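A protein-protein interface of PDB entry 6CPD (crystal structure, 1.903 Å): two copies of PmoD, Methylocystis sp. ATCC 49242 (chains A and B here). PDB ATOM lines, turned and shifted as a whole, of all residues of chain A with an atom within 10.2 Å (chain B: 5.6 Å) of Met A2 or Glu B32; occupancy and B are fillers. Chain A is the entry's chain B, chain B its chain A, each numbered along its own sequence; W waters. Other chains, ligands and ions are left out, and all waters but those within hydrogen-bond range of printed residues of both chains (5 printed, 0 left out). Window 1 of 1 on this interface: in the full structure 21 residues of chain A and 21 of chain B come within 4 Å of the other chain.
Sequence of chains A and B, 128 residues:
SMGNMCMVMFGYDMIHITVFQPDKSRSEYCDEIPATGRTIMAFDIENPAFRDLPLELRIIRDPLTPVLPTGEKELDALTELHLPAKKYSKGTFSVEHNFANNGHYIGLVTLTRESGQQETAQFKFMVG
NE2 of His A16 sits at hydrogen-bond distance from OD2 of Asp B31.
The side-chain sulfur of Met A5 lies close to the backbone carbonyl oxygen of Lys B124 (3.6 Å).
OD2 of Asp B31 lies within hydrogen-bond range of N of Met A5.
The backbone NH of Cys A6 lies within hydrogen-bond range of the side-chain carboxylate of Asp B31.
A ring nitrogen (NE2) of His B104 sits at hydrogen-bond distance from the side-chain sulfur (SD) of Met A2 (3.4 Å).
OD1 of Asn A4 is in hydrogen-bond range of N of Lys B124 (2.8 Å).
OE1 of Glu A28 sits close to OE1 of Glu B32 (2.7 Å).
The backbone carbonyl oxygen of Cys A6 is in hydrogen-bond range of the backbone NH of Ile A17 (2.9 Å).
The side-chain sulfur (SG) of Cys A6 forms a disulfide with the side-chain sulfur (SG) of Cys A30 (2.1 Å).
OG of Ser A25 lies within hydrogen-bond range of N of Ser A27, at 2.7 Å.
A ring nitrogen (NE2) of His A16 lies within hydrogen-bond range of the backbone carbonyl oxygen (O) of Gly A3.
The backbone carbonyl oxygen (O) of Asp B31 sits at hydrogen-bond distance from the backbone NH (N) of Met B126 (2.8 Å).
N of Asp A44 is in hydrogen-bond range of O of His A16 (2.8 Å).
Among the printed residues, pairs that only touch across the chains: Met A2 with Glu B32, Gly A3 with Asp B31, Gly A3 with Lys B124, Asn A4 with Asp B31, Met A5 with Cys B30, Cys A6 with Cys B30, Ser A27 with Pro B34, Glu A28 with Tyr B29 and Cys A30 with Cys B30.
Met A2 touches two residues of chain B.
Of the printed residues of chain B, Asn A4 touches Asp B31 (3.5 Å) and Lys B124 (2.8 Å).
Of the printed residues of chain B, Glu A28 touches Tyr B29 (3.8 Å) and Glu B32 (2.7 Å).
Glu A46 touches none of the printed residues of chain B.
Printed residues of chain A within 4 Å of Cys B30: Met A5 (3.5 Å), Cys A6 (3.8 Å) and Cys A30 (3.5 Å).
Asp B31 touches five residues of chain A.
Glu B32 touches two residues of chain A.
No residue of chain A comes within 4 Å of Ile B33.
Of the printed residues of chain A, Pro B34 touches Ser A27.
Lys B124 touches three residues of chain A.
No residue of chain A comes within 4 Å of Met B126.
Of the 11 printed residues of chain B, 7 touch a printed residue of chain A.
Hydrophobic or aromatic side chains of chain A that line the printed part of chain B: Met A2, Met A5 and His A16.
Among the printed residues, 16 pairs touch across the chains.
Among the printed residues, no Asp or Glu carboxylate lies within 4 Å of a Lys or Arg side-chain nitrogen of the other chain.
Cys A30 touches its own counterpart, Cys B30.
4 positions are printed for both chains.
Of the 16 pairs that touch across the chains among the printed residues, 1 has its exchanged pair printed and touching as well.
Water W5 bridges the backbone carbonyl oxygen of Glu B32 (2.7 Å) and the backbone NH of Glu A28 (2.8 Å).
Water W4 lies within hydrogen-bond range of O of Glu A28, N of Cys B30 and O of Glu B32.
Water W1 lies within hydrogen-bond range of the backbone NH of Gly A3 (2.7 Å), the side-chain carboxylate of Glu B32 (3.1 Å), the backbone carbonyl oxygen of Asp B31 (3.3 Å) and the backbone NH of Met B126 (3.4 Å).
Water W3 lies within hydrogen-bond range of O of Ile A17, OD1 of Asp B31, OG1 of Thr A18 and NE2 of His A16.
Water W2 lies within hydrogen-bond range of the backbone carbonyl oxygen of Tyr A29 and the side-chain carboxylate of Asp B31.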
ATOM      1  N   MET A   2     -30.537   5.653  17.463  1.00  0.00           N
ATOM      2  CA  MET A   2     -29.634   4.510  17.557  1.00  0.00           C
ATOM      3  C   MET A   2     -30.276   3.334  18.306  1.00  0.00           C
ATOM      4  O   MET A   2     -31.169   2.650  17.775  1.00  0.00           O
ATOM      5  CB  MET A   2     -28.330   4.914  18.252  1.00  0.00           C
ATOM      6  CG  MET A   2     -27.407   5.795  17.421  1.00  0.00           C
ATOM      7  SD  MET A   2     -27.030   5.119  15.789  1.00  0.00           S
ATOM      8  CE  MET A   2     -25.624   6.131  15.326  1.00  0.00           C
ATOM      9  N   GLY A   3     -29.801   3.104  19.531  1.00  0.00           N
ATOM     10  CA  GLY A   3     -30.319   2.053  20.394  1.00  0.00           C
ATOM     11  C   GLY A   3     -31.743   2.355  20.803  1.00  0.00           C
ATOM     12  O   GLY A   3     -32.168   3.504  20.781  1.00  0.00           O
ATOM     13  N   ASN A   4     -32.506   1.326  21.161  1.00  0.00           N
ATOM     14  CA  ASN A   4     -33.811   1.543  21.779  1.00  0.00           C
ATOM     15  C   ASN A   4     -33.976   0.963  23.176  1.00  0.00           C
ATOM     16  O   ASN A   4     -35.111   0.762  23.614  1.00  0.00           O
ATOM     17  CB  ASN A   4     -34.915   0.996  20.867  1.00  0.00           C
ATOM     18  CG  ASN A   4     -34.953  -0.516  20.844  1.00  0.00           C
ATOM     19  OD1 ASN A   4     -34.016  -1.191  21.310  1.00  0.00           O
ATOM     20  ND2 ASN A   4     -36.027  -1.065  20.289  1.00  0.00           N
ATOM     21  N   MET A   5     -32.881   0.641  23.867  1.00  0.00           N
ATOM     22  CA  MET A   5     -33.014  -0.199  25.066  1.00  0.00           C
ATOM     23  C   MET A   5     -32.978   0.561  26.382  1.00  0.00           C
ATOM     24  O   MET A   5     -33.595   0.143  27.355  1.00  0.00           O
ATOM     25  CB  MET A   5     -31.890  -1.243  25.067  1.00  0.00           C
ATOM     26  CG  MET A   5     -31.962  -2.208  23.901  1.00  0.00           C
ATOM     27  SD  MET A   5     -30.394  -3.091  23.694  1.00  0.00           S
ATOM     28  CE  MET A   5     -30.387  -3.945  25.266  1.00  0.00           C
ATOM     29  N   CYS A   6     -32.297   1.701  26.403  1.00  0.00           N
ATOM     30  CA  CYS A   6     -32.124   2.461  27.635  1.00  0.00           C
ATOM     31  C   CYS A   6     -33.194   3.535  27.715  1.00  0.00           C
ATOM     32  O   CYS A   6     -33.194   4.433  26.895  1.00  0.00           O
ATOM     33  CB  CYS A   6     -30.724   3.098  27.680  1.00  0.00           C
ATOM     34  SG  CYS A   6     -30.411   4.075  29.190  1.00  0.00           S
ATOM     35  N   HIS A  16     -35.713   7.844  25.263  1.00  0.00           N
ATOM     36  CA  HIS A  16     -34.465   7.104  25.229  1.00  0.00           C
ATOM     37  C   HIS A  16     -33.381   7.951  25.873  1.00  0.00           C
ATOM     38  O   HIS A  16     -33.329   9.172  25.690  1.00  0.00           O
ATOM     39  CB  HIS A  16     -34.079   6.745  23.790  1.00  0.00           C
ATOM     40  CG  HIS A  16     -32.830   5.934  23.686  1.00  0.00           C
ATOM     41  ND1 HIS A  16     -31.621   6.475  23.299  1.00  0.00           N
ATOM     42  CD2 HIS A  16     -32.595   4.621  23.929  1.00  0.00           C
ATOM     43  CE1 HIS A  16     -30.698   5.529  23.298  1.00  0.00           C
ATOM     44  NE2 HIS A  16     -31.264   4.395  23.672  1.00  0.00           N
ATOM     45  N   ILE A  17     -32.505   7.286  26.600  1.00  0.00           N
ATOM     46  CA  ILE A  17     -31.433   7.955  27.348  1.00  0.00           C
ATOM     47  C   ILE A  17     -30.071   7.365  26.984  1.00  0.00           C
ATOM     48  O   ILE A  17     -29.927   6.138  26.897  1.00  0.00           O
ATOM     49  CB  ILE A  17     -31.659   7.797  28.869  1.00  0.00           C
ATOM     50  CG1 ILE A  17     -32.967   8.487  29.278  1.00  0.00           C
ATOM     51  CG2 ILE A  17     -30.468   8.362  29.659  1.00  0.00           C
ATOM     52  CD1 ILE A  17     -33.388   8.180  30.720  1.00  0.00           C
ATOM     53  N   THR A  18     -29.082   8.235  26.783  1.00  0.00           N
ATOM     54  CA  THR A  18     -27.700   7.823  26.591  1.00  0.00           C
ATOM     55  C   THR A  18     -26.825   8.593  27.594  1.00  0.00           C
ATOM     56  O   THR A  18     -27.048   9.779  27.840  1.00  0.00           O
ATOM     57  CB  THR A  18     -27.189   8.107  25.151  1.00  0.00           C
ATOM     58  OG1 THR A  18     -28.086   7.546  24.179  1.00  0.00           O
ATOM     59  CG2 THR A  18     -25.804   7.514  24.954  1.00  0.00           C
ATOM     60  N   VAL A  19     -25.857   7.912  28.185  1.00  0.00           N
ATOM     61  CA  VAL A  19     -24.962   8.550  29.136  1.00  0.00           C
ATOM     62  C   VAL A  19     -23.532   8.390  28.681  1.00  0.00           C
ATOM     63  O   VAL A  19     -23.121   7.277  28.345  1.00  0.00           O
ATOM     64  CB  VAL A  19     -25.105   7.931  30.544  1.00  0.00           C
ATOM     65  CG1 VAL A  19     -24.238   8.677  31.534  1.00  0.00           C
ATOM     66  CG2 VAL A  19     -26.574   7.941  30.994  1.00  0.00           C
ATOM     67  N   PHE A  20     -22.763   9.476  28.626  1.00  0.00           N
ATOM     68  CA  PHE A  20     -21.332   9.279  28.430  1.00  0.00           C
ATOM     69  C   PHE A  20     -20.509  10.142  29.382  1.00  0.00           C
ATOM     70  O   PHE A  20     -21.014  11.090  29.983  1.00  0.00           O
ATOM     71  CB  PHE A  20     -20.901   9.458  26.966  1.00  0.00           C
ATOM     72  CG  PHE A  20     -21.092  10.821  26.399  1.00  0.00           C
ATOM     73  CD1 PHE A  20     -22.338  11.225  25.941  1.00  0.00           C
ATOM     74  CD2 PHE A  20     -19.991  11.660  26.197  1.00  0.00           C
ATOM     75  CE1 PHE A  20     -22.503  12.481  25.358  1.00  0.00           C
ATOM     76  CE2 PHE A  20     -20.142  12.919  25.615  1.00  0.00           C
ATOM     77  CZ  PHE A  20     -21.403  13.328  25.192  1.00  0.00           C
ATOM     78  N   SER A  25     -13.719   7.987  29.095  1.00  0.00           N
ATOM     79  CA  SER A  25     -13.913   6.965  28.093  1.00  0.00           C
ATOM     80  C   SER A  25     -14.718   7.457  26.889  1.00  0.00           C
ATOM     81  O   SER A  25     -15.391   8.473  26.960  1.00  0.00           O
ATOM     82  CB  SER A  25     -14.614   5.775  28.758  1.00  0.00           C
ATOM     83  OG  SER A  25     -15.269   4.960  27.821  1.00  0.00           O
ATOM     84  N   ARG A  26     -14.647   6.723  25.784  1.00  0.00           N
ATOM     85  CA  ARG A  26     -15.498   6.988  24.630  1.00  0.00           C
ATOM     86  C   ARG A  26     -16.710   6.053  24.610  1.00  0.00           C
ATOM     87  O   ARG A  26     -17.458   6.025  23.630  1.00  0.00           O
ATOM     88  CB  ARG A  26     -14.707   6.853  23.322  1.00  0.00           C
ATOM     89  CG  ARG A  26     -13.596   7.900  23.107  1.00  0.00           C
ATOM     90  CD  ARG A  26     -14.157   9.340  23.115  1.00  0.00           C
ATOM     91  NE  ARG A  26     -13.116  10.375  23.142  1.00  0.00           N
ATOM     92  CZ  ARG A  26     -12.910  11.172  24.188  1.00  0.00           C
ATOM     93  NH1 ARG A  26     -13.684  11.047  25.268  1.00  0.00           N
ATOM     94  NH2 ARG A  26     -11.941  12.080  24.168  1.00  0.00           N
ATOM     95  N   SER A  27     -16.889   5.276  25.680  1.00  0.00           N
ATOM     96  CA  SER A  27     -18.027   4.361  25.785  1.00  0.00           C
ATOM     97  C   SER A  27     -19.335   5.082  26.148  1.00  0.00           C
ATOM     98  O   SER A  27     -19.330   6.227  26.606  1.00  0.00           O
ATOM     99  CB  SER A  27     -17.754   3.274  26.838  1.00  0.00           C
ATOM    100  OG  SER A  27     -16.550   2.572  26.575  1.00  0.00           O
ATOM    101  N   GLU A  28     -20.454   4.390  25.974  1.00  0.00           N
ATOM    102  CA  GLU A  28     -21.764   4.922  26.350  1.00  0.00           C
ATOM    103  C   GLU A  28     -22.398   4.004  27.379  1.00  0.00           C
ATOM    104  O   GLU A  28     -22.260   2.792  27.276  1.00  0.00           O
ATOM    105  CB  GLU A  28     -22.677   5.044  25.133  1.00  0.00           C
ATOM    106  CG  GLU A  28     -22.164   5.989  24.075  1.00  0.00           C
ATOM    107  CD  GLU A  28     -22.929   5.858  22.770  1.00  0.00           C
ATOM    108  OE1 GLU A  28     -22.341   5.355  21.790  1.00  0.00           O
ATOM    109  OE2 GLU A  28     -24.131   6.199  22.735  1.00  0.00           O
ATOM    110  N   TYR A  29     -23.086   4.571  28.360  1.00  0.00           N
ATOM    111  CA  TYR A  29     -23.654   3.768  29.441  1.00  0.00           C
ATOM    112  C   TYR A  29     -25.153   3.993  29.576  1.00  0.00           C
ATOM    113  O   TYR A  29     -25.728   4.820  28.869  1.00  0.00           O
ATOM    114  CB  TYR A  29     -22.962   4.097  30.753  1.00  0.00           C
ATOM    115  CG  TYR A  29     -21.465   4.141  30.633  1.00  0.00           C
ATOM    116  CD1 TYR A  29     -20.711   2.973  30.668  1.00  0.00           C
ATOM    117  CD2 TYR A  29     -20.803   5.353  30.468  1.00  0.00           C
ATOM    118  CE1 TYR A  29     -19.326   3.017  30.555  1.00  0.00           C
ATOM    119  CE2 TYR A  29     -19.412   5.409  30.355  1.00  0.00           C
ATOM    120  CZ  TYR A  29     -18.689   4.237  30.405  1.00  0.00           C
ATOM    121  OH  TYR A  29     -17.327   4.291  30.284  1.00  0.00           O
ATOM    122  N   CYS A  30     -25.778   3.264  30.495  1.00  0.00           N
ATOM    123  CA  CYS A  30     -27.198   3.445  30.749  1.00  0.00           C
ATOM    124  C   CYS A  30     -27.389   3.669  32.249  1.00  0.00           C
ATOM    125  O   CYS A  30     -27.304   4.805  32.711  1.00  0.00           O
ATOM    126  CB  CYS A  30     -28.021   2.254  30.244  1.00  0.00           C
ATOM    127  SG  CYS A  30     -29.841   2.511  30.401  1.00  0.00           S
ATOM    128  N   ASP A  31     -27.661   2.615  33.019  1.00  0.00           N
ATOM    129  CA  ASP A  31     -27.960   2.845  34.430  1.00  0.00           C
ATOM    130  C   ASP A  31     -26.811   2.456  35.359  1.00  0.00           C
ATOM    131  O   ASP A  31     -26.941   2.551  36.576  1.00  0.00           O
ATOM    132  CB  ASP A  31     -29.230   2.109  34.851  1.00  0.00           C
ATOM    133  CG  ASP A  31     -29.235   0.664  34.427  1.00  0.00           C
ATOM    134  OD1 ASP A  31     -28.141   0.098  34.244  1.00  0.00           O
ATOM    135  OD2 ASP A  31     -30.336   0.091  34.296  1.00  0.00           O
ATOM    136  N   GLU A  32     -25.693   2.036  34.778  1.00  0.00           N
ATOM    137  CA  GLU A  32     -24.493   1.757  35.558  1.00  0.00           C
ATOM    138  C   GLU A  32     -23.392   2.644  35.026  1.00  0.00           C
ATOM    139  O   GLU A  32     -22.748   2.326  34.026  1.00  0.00           O
ATOM    140  CB  GLU A  32     -24.108   0.289  35.459  1.00  0.00           C
ATOM    141  CG  GLU A  32     -25.226  -0.656  35.861  1.00  0.00           C
ATOM    142  CD  GLU A  32     -25.271  -0.889  37.361  1.00  0.00           C
ATOM    143  OE1 GLU A  32     -24.225  -0.707  38.023  1.00  0.00           O
ATOM    144  OE2 GLU A  32     -26.354  -1.243  37.874  1.00  0.00           O
ATOM    145  N   ASP A  44     -33.881  11.551  24.281  1.00  0.00           N
ATOM    146  CA  ASP A  44     -34.499  11.534  22.958  1.00  0.00           C
ATOM    147  C   ASP A  44     -35.960  11.095  23.150  1.00  0.00           C
ATOM    148  O   ASP A  44     -36.246   9.922  23.391  1.00  0.00           O
ATOM    149  CB  ASP A  44     -33.765  10.558  22.028  1.00  0.00           C
ATOM    150  CG  ASP A  44     -34.380  10.479  20.620  1.00  0.00           C
ATOM    151  OD1 ASP A  44     -35.492  11.002  20.378  1.00  0.00           O
ATOM    152  OD2 ASP A  44     -33.763   9.815  19.758  1.00  0.00           O
ATOM    153  N   GLU A  46     -39.388   9.786  22.221  1.00  0.00           N
ATOM    154  CA  GLU A  46     -39.852   8.988  21.087  1.00  0.00           C
ATOM    155  C   GLU A  46     -41.160   9.486  20.465  1.00  0.00           C
ATOM    156  O   GLU A  46     -41.322   9.418  19.254  1.00  0.00           O
ATOM    157  CB  GLU A  46     -40.029   7.513  21.486  1.00  0.00           C
ATOM    158  CG  GLU A  46     -38.712   6.759  21.684  1.00  0.00           C
ATOM    159  CD  GLU A  46     -38.903   5.255  21.892  1.00  0.00           C
ATOM    160  OE1 GLU A  46     -40.052   4.804  22.115  1.00  0.00           O
ATOM    161  OE2 GLU A  46     -37.899   4.520  21.805  1.00  0.00           O
ATOM    162  N   THR A  92     -35.286  16.525  21.658  1.00  0.00           N
ATOM    163  CA  THR A  92     -34.031  16.056  22.228  1.00  0.00           C
ATOM    164  C   THR A  92     -33.438  17.128  23.128  1.00  0.00           C
ATOM    165  O   THR A  92     -33.687  18.317  22.932  1.00  0.00           O
ATOM    166  CB  THR A  92     -32.989  15.687  21.136  1.00  0.00           C
ATOM    167  OG1 THR A  92     -32.663  16.851  20.361  1.00  0.00           O
ATOM    168  CG2 THR A  92     -33.520  14.598  20.215  1.00  0.00           C
ATOM    169  N   TYR B  29     -22.900  -2.208  30.027  1.00  0.00           N
ATOM    170  CA  TYR B  29     -23.390  -1.444  28.895  1.00  0.00           C
ATOM    171  C   TYR B  29     -24.842  -1.806  28.611  1.00  0.00           C
ATOM    172  O   TYR B  29     -25.415  -2.724  29.237  1.00  0.00           O
ATOM    173  CB  TYR B  29     -22.515  -1.704  27.655  1.00  0.00           C
ATOM    174  CG  TYR B  29     -21.013  -1.635  27.939  1.00  0.00           C
ATOM    175  CD1 TYR B  29     -20.368  -0.416  28.044  1.00  0.00           C
ATOM    176  CD2 TYR B  29     -20.249  -2.791  28.079  1.00  0.00           C
ATOM    177  CE1 TYR B  29     -18.988  -0.338  28.311  1.00  0.00           C
ATOM    178  CE2 TYR B  29     -18.876  -2.726  28.339  1.00  0.00           C
ATOM    179  CZ  TYR B  29     -18.258  -1.495  28.440  1.00  0.00           C
ATOM    180  OH  TYR B  29     -16.914  -1.409  28.701  1.00  0.00           O
ATOM    181  N   CYS B  30     -25.440  -1.091  27.667  1.00  0.00           N
ATOM    182  CA  CYS B  30     -26.805  -1.380  27.285  1.00  0.00           C
ATOM    183  C   CYS B  30     -26.866  -1.498  25.764  1.00  0.00           C
ATOM    184  O   CYS B  30     -26.567  -2.560  25.221  1.00  0.00           O
ATOM    185  CB  CYS B  30     -27.761  -0.307  27.820  1.00  0.00           C
ATOM    186  SG  CYS B  30     -29.525  -0.639  27.540  1.00  0.00           S
ATOM    187  N   ASP B  31     -27.211  -0.427  25.056  1.00  0.00           N
ATOM    188  CA  ASP B  31     -27.384  -0.599  23.604  1.00  0.00           C
ATOM    189  C   ASP B  31     -26.203  -0.061  22.787  1.00  0.00           C
ATOM    190  O   ASP B  31     -26.220  -0.064  21.557  1.00  0.00           O
ATOM    191  CB  ASP B  31     -28.718   0.005  23.133  1.00  0.00           C
ATOM    192  CG  ASP B  31     -28.989   1.368  23.707  1.00  0.00           C
ATOM    193  OD1 ASP B  31     -28.029   2.072  24.066  1.00  0.00           O
ATOM    194  OD2 ASP B  31     -30.183   1.730  23.779  1.00  0.00           O
ATOM    195  N   GLU B  32     -25.145   0.313  23.490  1.00  0.00           N
ATOM    196  CA  GLU B  32     -23.893   0.696  22.850  1.00  0.00           C
ATOM    197  C   GLU B  32     -22.719  -0.128  23.391  1.00  0.00           C
ATOM    198  O   GLU B  32     -22.207   0.151  24.469  1.00  0.00           O
ATOM    199  CB  GLU B  32     -23.652   2.191  23.059  1.00  0.00           C
ATOM    200  CG  GLU B  32     -24.838   3.057  22.615  1.00  0.00           C
ATOM    201  CD  GLU B  32     -24.813   3.389  21.128  1.00  0.00           C
ATOM    202  OE1 GLU B  32     -23.713   3.351  20.534  1.00  0.00           O
ATOM    203  OE2 GLU B  32     -25.888   3.687  20.555  1.00  0.00           O
ATOM    204  N   ILE B  33     -22.306  -1.144  22.647  1.00  0.00           N
ATOM    205  CA  ILE B  33     -21.197  -1.998  23.038  1.00  0.00           C
ATOM    206  C   ILE B  33     -19.894  -1.394  22.460  1.00  0.00           C
ATOM    207  O   ILE B  33     -19.799  -1.160  21.259  1.00  0.00           O
ATOM    208  CB  ILE B  33     -21.424  -3.428  22.547  1.00  0.00           C
ATOM    209  CG1 ILE B  33     -22.761  -3.947  23.105  1.00  0.00           C
ATOM    210  CG2 ILE B  33     -20.276  -4.323  22.960  1.00  0.00           C
ATOM    211  CD1 ILE B  33     -23.242  -5.226  22.445  1.00  0.00           C
ATOM    212  N   PRO B  34     -18.927  -1.053  23.324  1.00  0.00           N
ATOM    213  CA  PRO B  34     -17.895  -0.152  22.795  1.00  0.00           C
ATOM    214  C   PRO B  34     -16.913  -0.804  21.826  1.00  0.00           C
ATOM    215  O   PRO B  34     -16.361  -0.105  20.973  1.00  0.00           O
ATOM    216  CB  PRO B  34     -17.150   0.309  24.059  1.00  0.00           C
ATOM    217  CG  PRO B  34     -17.373  -0.777  25.055  1.00  0.00           C
ATOM    218  CD  PRO B  34     -18.761  -1.311  24.766  1.00  0.00           C
ATOM    219  N   HIS B 104     -24.573  -2.059  13.354  1.00  0.00           N
ATOM    220  CA  HIS B 104     -25.860  -2.054  14.041  1.00  0.00           C
ATOM    221  C   HIS B 104     -26.439  -3.454  14.040  1.00  0.00           C
ATOM    222  O   HIS B 104     -26.321  -4.187  13.052  1.00  0.00           O
ATOM    223  CB  HIS B 104     -26.816  -1.065  13.366  1.00  0.00           C
ATOM    224  CG  HIS B 104     -26.354   0.356  13.457  1.00  0.00           C
ATOM    225  ND1 HIS B 104     -25.593   0.956  12.481  1.00  0.00           N
ATOM    226  CD2 HIS B 104     -26.534   1.290  14.420  1.00  0.00           C
ATOM    227  CE1 HIS B 104     -25.319   2.197  12.836  1.00  0.00           C
ATOM    228  NE2 HIS B 104     -25.877   2.425  14.012  1.00  0.00           N
ATOM    229  N   LYS B 124     -32.603  -2.997  19.719  1.00  0.00           N
ATOM    230  CA  LYS B 124     -31.605  -2.487  18.797  1.00  0.00           C
ATOM    231  C   LYS B 124     -30.375  -2.013  19.547  1.00  0.00           C
ATOM    232  O   LYS B 124     -30.492  -1.294  20.546  1.00  0.00           O
ATOM    233  CB  LYS B 124     -32.193  -1.345  17.972  1.00  0.00           C
ATOM    234  CG  LYS B 124     -33.376  -1.777  17.146  1.00  0.00           C
ATOM    235  CD  LYS B 124     -33.646  -0.730  16.062  1.00  0.00           C
ATOM    236  CE  LYS B 124     -34.725  -1.196  15.115  1.00  0.00           C
ATOM    237  NZ  LYS B 124     -34.837  -0.296  13.943  1.00  0.00           N
ATOM    238  N   PHE B 125     -29.201  -2.388  19.050  1.00  0.00           N
ATOM    239  CA  PHE B 125     -27.958  -1.975  19.680  1.00  0.00           C
ATOM    240  C   PHE B 125     -26.866  -1.854  18.643  1.00  0.00           C
ATOM    241  O   PHE B 125     -27.038  -2.241  17.491  1.00  0.00           O
ATOM    242  CB  PHE B 125     -27.536  -2.951  20.799  1.00  0.00           C
ATOM    243  CG  PHE B 125     -27.225  -4.346  20.331  1.00  0.00           C
ATOM    244  CD1 PHE B 125     -25.908  -4.755  20.166  1.00  0.00           C
ATOM    245  CD2 PHE B 125     -28.244  -5.269  20.107  1.00  0.00           C
ATOM    246  CE1 PHE B 125     -25.599  -6.069  19.756  1.00  0.00           C
ATOM    247  CE2 PHE B 125     -27.950  -6.570  19.704  1.00  0.00           C
ATOM    248  CZ  PHE B 125     -26.616  -6.972  19.536  1.00  0.00           C
ATOM    249  N   MET B 126     -25.744  -1.283  19.042  1.00  0.00           N
ATOM    250  CA  MET B 126     -24.618  -1.221  18.118  1.00  0.00           C
ATOM    251  C   MET B 126     -23.299  -1.584  18.794  1.00  0.00           C
ATOM    252  O   MET B 126     -23.159  -1.506  20.029  1.00  0.00           O
ATOM    253  CB  MET B 126     -24.570   0.159  17.478  1.00  0.00           C
ATOM    254  CG  MET B 126     -24.225   1.269  18.398  1.00  0.00           C
ATOM    255  SD  MET B 126     -23.954   2.788  17.453  1.00  0.00           S
ATOM    256  CE  MET B 126     -22.777   2.203  16.242  1.00  0.00           C
ATOM    257  N   GLY B 128     -19.159  -0.881  18.635  1.00  0.00           N
ATOM    258  CA  GLY B 128     -18.066  -0.063  18.142  1.00  0.00           C
ATOM    259  C   GLY B 128     -18.465   1.384  17.944  1.00  0.00           C
ATOM    260  O   GLY B 128     -19.648   1.724  18.047  1.00  0.00           O
HETATM  261  O   HOH W   1     -27.599   1.546  19.011  1.00  0.00           O
HETATM  262  O   HOH W   2     -26.586   2.908  26.692  1.00  0.00           O
HETATM  263  O   HOH W   3     -28.282   4.544  25.349  1.00  0.00           O
HETATM  264  O   HOH W   4     -24.305   1.173  26.470  1.00  0.00           O
HETATM  265  O   HOH W   5     -20.188   1.959  24.546  1.00  0.00           O
